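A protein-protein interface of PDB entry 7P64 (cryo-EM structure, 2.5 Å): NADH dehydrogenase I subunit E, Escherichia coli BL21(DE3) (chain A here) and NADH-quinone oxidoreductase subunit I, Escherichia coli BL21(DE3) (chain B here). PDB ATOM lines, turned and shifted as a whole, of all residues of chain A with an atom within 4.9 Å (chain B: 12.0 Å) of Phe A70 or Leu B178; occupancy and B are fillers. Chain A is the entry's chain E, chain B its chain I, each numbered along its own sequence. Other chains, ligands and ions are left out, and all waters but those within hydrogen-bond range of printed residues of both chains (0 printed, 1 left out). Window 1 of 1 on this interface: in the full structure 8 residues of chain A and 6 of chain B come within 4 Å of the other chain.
OE1 of Gln A72 lies close to O of Lys B176 (3.5 Å).
The backbone NH (N) of Phe A70 sits at hydrogen-bond distance from the side-chain amide oxygen (OE1) of Gln A34 (2.5 Å).
The backbone NH (N) of Lys B176 sits close to the side-chain carboxylate (OD1) of Asp B174, at 3.3 Å.
The guanidinium group (NH1) of Arg A71 lies within hydrogen-bond range of the backbone carbonyl oxygen (O) of Val A40, at 2.9 Å.
O of Phe A70 is in hydrogen-bond range of N of Val A40, at 2.8 Å.
The backbone carbonyl oxygen of Asp B174 lies within hydrogen-bond range of the side-chain hydroxyl of Ser B177 (3.0 Å).
Phe A70 touches Leu B178.
Arg A71 touches Lys B176 (NH2 to CD, 3.7 Å).
Gln A72 touches Ser B177.
O of Gln A72 touches CD2 of Leu B178, 3.6 Å away.
Val A74 touches Leu B178 (CG1 to CD2, 3.7 Å).
Gly A108 touches Leu B179 (CA to CD2, 3.8 Å).
Leu B178 touches Leu A119 (O to CD2, 3.5 Å).
Of chain A, only Phe A70, Gln A72, Val A74 and Leu A119 come within 4 Å of Leu B178.
Gln A34 touches none of the printed residues of chain B.
No residue of chain B comes within 4 Å of Gly A38.
No residue of chain B comes within 4 Å of Trp A39.
No residue of chain B comes within 4 Å of Val A40.
Ile A69 touches none of the printed residues of chain B.
Arg A71 touches just one residue of chain B: Lys B176.
No residue of chain B comes within 4 Å of Pro A73.
Of chain B, only Leu B178 (3.7 Å) comes within 4 Å of Val A74.
Printed residues of chain A within 4 Å of Lys B176: Arg A71 (3.7 Å) and Gln A72 (3.4 Å).
Printed residues of chain A within 4 Å of Leu B179: Gly A108.
The nearest residue of chain B that does not touch Phe A70 is Lys B176 (5.4 Å).
The nearest residue of chain A that does not touch Leu B178 is Gly A108 (4.3 Å).
The nearest printed residue of chain A that does not touch Ser B177 is Arg A71 (5.8 Å).
Among the printed residues, 8 pairs touch across the chains.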
ATOM      1  N   GLN A  34     -17.805  22.387  23.487  1.00  0.00           N
ATOM      2  CA  GLN A  34     -17.832  20.944  23.278  1.00  0.00           C
ATOM      3  C   GLN A  34     -18.779  20.555  22.147  1.00  0.00           C
ATOM      4  O   GLN A  34     -18.464  19.672  21.346  1.00  0.00           O
ATOM      5  CB  GLN A  34     -18.229  20.244  24.576  1.00  0.00           C
ATOM      6  CG  GLN A  34     -18.413  18.749  24.451  1.00  0.00           C
ATOM      7  CD  GLN A  34     -18.167  18.028  25.751  1.00  0.00           C
ATOM      8  OE1 GLN A  34     -17.061  18.049  26.284  1.00  0.00           O
ATOM      9  NE2 GLN A  34     -19.202  17.386  26.275  1.00  0.00           N
ATOM     10  N   GLY A  38     -16.602  18.931  19.535  1.00  0.00           N
ATOM     11  CA  GLY A  38     -16.502  17.575  20.033  1.00  0.00           C
ATOM     12  C   GLY A  38     -15.990  17.470  21.455  1.00  0.00           C
ATOM     13  O   GLY A  38     -16.422  16.585  22.199  1.00  0.00           O
ATOM     14  N   TRP A  39     -15.085  18.359  21.848  1.00  0.00           N
ATOM     15  CA  TRP A  39     -14.491  18.364  23.177  1.00  0.00           C
ATOM     16  C   TRP A  39     -14.001  19.778  23.455  1.00  0.00           C
ATOM     17  O   TRP A  39     -14.218  20.696  22.660  1.00  0.00           O
ATOM     18  CB  TRP A  39     -13.362  17.334  23.289  1.00  0.00           C
ATOM     19  CG  TRP A  39     -12.172  17.618  22.419  1.00  0.00           C
ATOM     20  CD1 TRP A  39     -12.146  17.674  21.057  1.00  0.00           C
ATOM     21  CD2 TRP A  39     -10.831  17.867  22.854  1.00  0.00           C
ATOM     22  NE1 TRP A  39     -10.877  17.953  20.619  1.00  0.00           N
ATOM     23  CE2 TRP A  39     -10.050  18.073  21.703  1.00  0.00           C
ATOM     24  CE3 TRP A  39     -10.217  17.939  24.107  1.00  0.00           C
ATOM     25  CZ2 TRP A  39      -8.688  18.348  21.766  1.00  0.00           C
ATOM     26  CZ3 TRP A  39      -8.864  18.210  24.167  1.00  0.00           C
ATOM     27  CH2 TRP A  39      -8.114  18.411  23.004  1.00  0.00           C
ATOM     28  N   VAL A  40     -13.339  19.952  24.592  1.00  0.00           N
ATOM     29  CA  VAL A  40     -12.835  21.253  25.013  1.00  0.00           C
ATOM     30  C   VAL A  40     -11.309  21.206  24.956  1.00  0.00           C
ATOM     31  O   VAL A  40     -10.677  20.602  25.835  1.00  0.00           O
ATOM     32  CB  VAL A  40     -13.330  21.623  26.417  1.00  0.00           C
ATOM     33  CG1 VAL A  40     -12.809  22.988  26.817  1.00  0.00           C
ATOM     34  CG2 VAL A  40     -14.847  21.592  26.467  1.00  0.00           C
ATOM     35  N   SER A  67     -18.124  15.220  34.363  1.00  0.00           N
ATOM     36  CA  SER A  67     -17.699  14.121  33.509  1.00  0.00           C
ATOM     37  C   SER A  67     -18.164  14.275  32.069  1.00  0.00           C
ATOM     38  O   SER A  67     -17.539  13.704  31.170  1.00  0.00           O
ATOM     39  CB  SER A  67     -18.206  12.797  34.079  1.00  0.00           C
ATOM     40  OG  SER A  67     -19.620  12.790  34.161  1.00  0.00           O
ATOM     41  N   GLN A  68     -19.233  15.026  31.823  1.00  0.00           N
ATOM     42  CA  GLN A  68     -19.756  15.191  30.474  1.00  0.00           C
ATOM     43  C   GLN A  68     -19.079  16.315  29.706  1.00  0.00           C
ATOM     44  O   GLN A  68     -19.455  16.573  28.559  1.00  0.00           O
ATOM     45  CB  GLN A  68     -21.269  15.427  30.516  1.00  0.00           C
ATOM     46  CG  GLN A  68     -22.135  14.191  30.810  1.00  0.00           C
ATOM     47  CD  GLN A  68     -21.418  12.851  30.653  1.00  0.00           C
ATOM     48  OE1 GLN A  68     -21.032  12.453  29.551  1.00  0.00           O
ATOM     49  NE2 GLN A  68     -21.236  12.154  31.767  1.00  0.00           N
ATOM     50  N   ILE A  69     -18.107  16.989  30.304  1.00  0.00           N
ATOM     51  CA  ILE A  69     -17.259  17.942  29.602  1.00  0.00           C
ATOM     52  C   ILE A  69     -15.930  17.247  29.346  1.00  0.00           C
ATOM     53  O   ILE A  69     -15.209  16.900  30.287  1.00  0.00           O
ATOM     54  CB  ILE A  69     -17.076  19.239  30.400  1.00  0.00           C
ATOM     55  CG1 ILE A  69     -18.402  19.987  30.496  1.00  0.00           C
ATOM     56  CG2 ILE A  69     -16.013  20.111  29.758  1.00  0.00           C
ATOM     57  CD1 ILE A  69     -18.429  21.033  31.574  1.00  0.00           C
ATOM     58  N   PHE A  70     -15.608  17.030  28.076  1.00  0.00           N
ATOM     59  CA  PHE A  70     -14.446  16.240  27.698  1.00  0.00           C
ATOM     60  C   PHE A  70     -13.238  17.150  27.529  1.00  0.00           C
ATOM     61  O   PHE A  70     -13.253  18.064  26.701  1.00  0.00           O
ATOM     62  CB  PHE A  70     -14.718  15.463  26.413  1.00  0.00           C
ATOM     63  CG  PHE A  70     -15.909  14.560  26.498  1.00  0.00           C
ATOM     64  CD1 PHE A  70     -16.115  13.772  27.615  1.00  0.00           C
ATOM     65  CD2 PHE A  70     -16.822  14.500  25.464  1.00  0.00           C
ATOM     66  CE1 PHE A  70     -17.211  12.941  27.698  1.00  0.00           C
ATOM     67  CE2 PHE A  70     -17.920  13.671  25.541  1.00  0.00           C
ATOM     68  CZ  PHE A  70     -18.115  12.891  26.659  1.00  0.00           C
ATOM     69  N   ARG A  71     -12.197  16.896  28.316  1.00  0.00           N
ATOM     70  CA  ARG A  71     -10.942  17.624  28.222  1.00  0.00           C
ATOM     71  C   ARG A  71      -9.870  16.831  27.490  1.00  0.00           C
ATOM     72  O   ARG A  71      -8.714  17.260  27.445  1.00  0.00           O
ATOM     73  CB  ARG A  71     -10.460  18.014  29.618  1.00  0.00           C
ATOM     74  CG  ARG A  71     -11.153  19.241  30.178  1.00  0.00           C
ATOM     75  CD  ARG A  71     -10.828  20.469  29.357  1.00  0.00           C
ATOM     76  NE  ARG A  71      -9.520  21.005  29.711  1.00  0.00           N
ATOM     77  CZ  ARG A  71      -8.458  20.968  28.919  1.00  0.00           C
ATOM     78  NH1 ARG A  71      -8.521  20.453  27.704  1.00  0.00           N
ATOM     79  NH2 ARG A  71      -7.304  21.455  29.361  1.00  0.00           N
ATOM     80  N   GLN A  72     -10.229  15.686  26.923  1.00  0.00           N
ATOM     81  CA  GLN A  72      -9.378  14.881  26.064  1.00  0.00           C
ATOM     82  C   GLN A  72     -10.126  14.598  24.772  1.00  0.00           C
ATOM     83  O   GLN A  72     -11.360  14.561  24.772  1.00  0.00           O
ATOM     84  CB  GLN A  72      -8.983  13.564  26.750  1.00  0.00           C
ATOM     85  CG  GLN A  72      -7.511  13.492  27.115  1.00  0.00           C
ATOM     86  CD  GLN A  72      -7.244  12.590  28.296  1.00  0.00           C
ATOM     87  OE1 GLN A  72      -7.932  11.591  28.498  1.00  0.00           O
ATOM     88  NE2 GLN A  72      -6.236  12.936  29.086  1.00  0.00           N
ATOM     89  N   PRO A  73      -9.415  14.427  23.654  1.00  0.00           N
ATOM     90  CA  PRO A  73     -10.104  14.237  22.366  1.00  0.00           C
ATOM     91  C   PRO A  73     -10.873  12.925  22.323  1.00  0.00           C
ATOM     92  O   PRO A  73     -10.367  11.876  22.725  1.00  0.00           O
ATOM     93  CB  PRO A  73      -8.960  14.252  21.344  1.00  0.00           C
ATOM     94  CG  PRO A  73      -7.737  13.946  22.130  1.00  0.00           C
ATOM     95  CD  PRO A  73      -7.960  14.556  23.473  1.00  0.00           C
ATOM     96  N   VAL A  74     -12.108  12.998  21.832  1.00  0.00           N
ATOM     97  CA  VAL A  74     -12.994  11.849  21.745  1.00  0.00           C
ATOM     98  C   VAL A  74     -13.265  11.553  20.275  1.00  0.00           C
ATOM     99  O   VAL A  74     -12.853  12.290  19.381  1.00  0.00           O
ATOM    100  CB  VAL A  74     -14.314  12.070  22.508  1.00  0.00           C
ATOM    101  CG1 VAL A  74     -14.041  12.334  23.971  1.00  0.00           C
ATOM    102  CG2 VAL A  74     -15.093  13.220  21.896  1.00  0.00           C
ATOM    103  N   VAL A  78     -19.978   9.163  20.586  1.00  0.00           N
ATOM    104  CA  VAL A  78     -19.681   8.781  21.961  1.00  0.00           C
ATOM    105  C   VAL A  78     -20.796   7.868  22.449  1.00  0.00           C
ATOM    106  O   VAL A  78     -21.948   8.298  22.588  1.00  0.00           O
ATOM    107  CB  VAL A  78     -19.532  10.004  22.875  1.00  0.00           C
ATOM    108  CG1 VAL A  78     -19.131   9.569  24.271  1.00  0.00           C
ATOM    109  CG2 VAL A  78     -18.514  10.970  22.303  1.00  0.00           C
ATOM    110  N   GLY A 108     -13.368   3.970  28.131  1.00  0.00           N
ATOM    111  CA  GLY A 108     -12.439   5.071  28.248  1.00  0.00           C
ATOM    112  C   GLY A 108     -11.499   5.229  27.074  1.00  0.00           C
ATOM    113  O   GLY A 108     -10.721   6.191  27.049  1.00  0.00           O
ATOM    114  N   THR A 117     -16.197   6.301  20.711  1.00  0.00           N
ATOM    115  CA  THR A 117     -15.574   6.391  22.025  1.00  0.00           C
ATOM    116  C   THR A 117     -16.510   5.733  23.027  1.00  0.00           C
ATOM    117  O   THR A 117     -17.649   6.178  23.198  1.00  0.00           O
ATOM    118  CB  THR A 117     -15.301   7.844  22.419  1.00  0.00           C
ATOM    119  OG1 THR A 117     -14.272   8.383  21.582  1.00  0.00           O
ATOM    120  CG2 THR A 117     -14.858   7.930  23.867  1.00  0.00           C
ATOM    121  N   LEU A 119     -17.764   4.704  26.734  1.00  0.00           N
ATOM    122  CA  LEU A 119     -17.704   5.267  28.066  1.00  0.00           C
ATOM    123  C   LEU A 119     -18.814   4.682  28.931  1.00  0.00           C
ATOM    124  O   LEU A 119     -19.975   4.600  28.482  1.00  0.00           O
ATOM    125  CB  LEU A 119     -17.828   6.792  28.019  1.00  0.00           C
ATOM    126  CG  LEU A 119     -16.573   7.602  27.696  1.00  0.00           C
ATOM    127  CD1 LEU A 119     -16.933   9.054  27.450  1.00  0.00           C
ATOM    128  CD2 LEU A 119     -15.561   7.483  28.818  1.00  0.00           C
ATOM    129  N   PRO B 172      -0.902   6.939  37.596  1.00  0.00           N
ATOM    130  CA  PRO B 172      -1.597   8.214  37.800  1.00  0.00           C
ATOM    131  C   PRO B 172      -2.690   8.433  36.768  1.00  0.00           C
ATOM    132  O   PRO B 172      -2.527   8.128  35.585  1.00  0.00           O
ATOM    133  CB  PRO B 172      -0.481   9.255  37.664  1.00  0.00           C
ATOM    134  CG  PRO B 172       0.593   8.572  36.911  1.00  0.00           C
ATOM    135  CD  PRO B 172       0.522   7.132  37.278  1.00  0.00           C
ATOM    136  N   ILE B 173      -3.816   8.957  37.237  1.00  0.00           N
ATOM    137  CA  ILE B 173      -4.973   9.245  36.399  1.00  0.00           C
ATOM    138  C   ILE B 173      -5.061  10.753  36.242  1.00  0.00           C
ATOM    139  O   ILE B 173      -5.165  11.482  37.237  1.00  0.00           O
ATOM    140  CB  ILE B 173      -6.267   8.675  36.999  1.00  0.00           C
ATOM    141  CG1 ILE B 173      -6.138   7.168  37.214  1.00  0.00           C
ATOM    142  CG2 ILE B 173      -7.447   8.986  36.105  1.00  0.00           C
ATOM    143  CD1 ILE B 173      -7.141   6.606  38.191  1.00  0.00           C
ATOM    144  N   ASP B 174      -5.006  11.220  35.001  1.00  0.00           N
ATOM    145  CA  ASP B 174      -5.124  12.643  34.729  1.00  0.00           C
ATOM    146  C   ASP B 174      -6.542  13.114  35.028  1.00  0.00           C
ATOM    147  O   ASP B 174      -7.513  12.369  34.880  1.00  0.00           O
ATOM    148  CB  ASP B 174      -4.763  12.934  33.272  1.00  0.00           C
ATOM    149  CG  ASP B 174      -4.368  14.383  33.037  1.00  0.00           C
ATOM    150  OD1 ASP B 174      -4.776  15.265  33.819  1.00  0.00           O
ATOM    151  OD2 ASP B 174      -3.642  14.642  32.057  1.00  0.00           O
ATOM    152  N   VAL B 175      -6.656  14.374  35.456  1.00  0.00           N
ATOM    153  CA  VAL B 175      -7.971  14.953  35.690  1.00  0.00           C
ATOM    154  C   VAL B 175      -8.713  15.201  34.385  1.00  0.00           C
ATOM    155  O   VAL B 175      -9.937  15.373  34.396  1.00  0.00           O
ATOM    156  CB  VAL B 175      -7.859  16.255  36.505  1.00  0.00           C
ATOM    157  CG1 VAL B 175      -7.414  15.952  37.921  1.00  0.00           C
ATOM    158  CG2 VAL B 175      -6.901  17.225  35.835  1.00  0.00           C
ATOM    159  N   LYS B 176      -8.008  15.214  33.257  1.00  0.00           N
ATOM    160  CA  LYS B 176      -8.619  15.379  31.947  1.00  0.00           C
ATOM    161  C   LYS B 176      -9.120  14.071  31.354  1.00  0.00           C
ATOM    162  O   LYS B 176      -9.648  14.081  30.239  1.00  0.00           O
ATOM    163  CB  LYS B 176      -7.622  16.024  30.983  1.00  0.00           C
ATOM    164  CG  LYS B 176      -7.055  17.340  31.465  1.00  0.00           C
ATOM    165  CD  LYS B 176      -6.329  18.057  30.345  1.00  0.00           C
ATOM    166  CE  LYS B 176      -4.844  18.151  30.622  1.00  0.00           C
ATOM    167  NZ  LYS B 176      -4.032  17.780  29.429  1.00  0.00           N
ATOM    168  N   SER B 177      -8.963  12.955  32.062  1.00  0.00           N
ATOM    169  CA  SER B 177      -9.383  11.659  31.547  1.00  0.00           C
ATOM    170  C   SER B 177     -10.902  11.578  31.440  1.00  0.00           C
ATOM    171  O   SER B 177     -11.639  12.168  32.233  1.00  0.00           O
ATOM    172  CB  SER B 177      -8.864  10.536  32.441  1.00  0.00           C
ATOM    173  OG  SER B 177      -9.527  10.535  33.691  1.00  0.00           O
ATOM    174  N   LEU B 178     -11.365  10.828  30.439  1.00  0.00           N
ATOM    175  CA  LEU B 178     -12.783  10.772  30.113  1.00  0.00           C
ATOM    176  C   LEU B 178     -13.588   9.900  31.065  1.00  0.00           C
ATOM    177  O   LEU B 178     -14.816  10.017  31.093  1.00  0.00           O
ATOM    178  CB  LEU B 178     -12.964  10.261  28.685  1.00  0.00           C
ATOM    179  CG  LEU B 178     -12.086  10.938  27.637  1.00  0.00           C
ATOM    180  CD1 LEU B 178     -12.102  10.153  26.342  1.00  0.00           C
ATOM    181  CD2 LEU B 178     -12.547  12.364  27.410  1.00  0.00           C
ATOM    182  N   LEU B 179     -12.936   9.033  31.829  1.00  0.00           N
ATOM    183  CA  LEU B 179     -13.660   8.126  32.705  1.00  0.00           C
ATOM    184  C   LEU B 179     -14.244   8.888  33.892  1.00  0.00           C
ATOM    185  O   LEU B 179     -13.565   9.730  34.487  1.00  0.00           O
ATOM    186  CB  LEU B 179     -12.741   7.012  33.196  1.00  0.00           C
ATOM    187  CG  LEU B 179     -12.487   5.886  32.196  1.00  0.00           C
ATOM    188  CD1 LEU B 179     -11.584   4.826  32.799  1.00  0.00           C
ATOM    189  CD2 LEU B 179     -13.801   5.277  31.748  1.00  0.00           C
ATOM    190  N   PRO B 180     -15.506   8.618  34.263  1.00  0.00           N
ATOM    191  CA  PRO B 180     -16.185   9.299  35.371  1.00  0.00           C
ATOM    192  C   PRO B 180     -15.553   9.004  36.729  1.00  0.00           C
ATOM    193  O   PRO B 180     -14.912   7.963  36.878  1.00  0.00           O
ATOM    194  CB  PRO B 180     -17.611   8.737  35.310  1.00  0.00           C
ATOM    195  CG  PRO B 180     -17.743   8.133  33.955  1.00  0.00           C
ATOM    196  CD  PRO B 180     -16.385   7.637  33.606  1.00  0.00           C
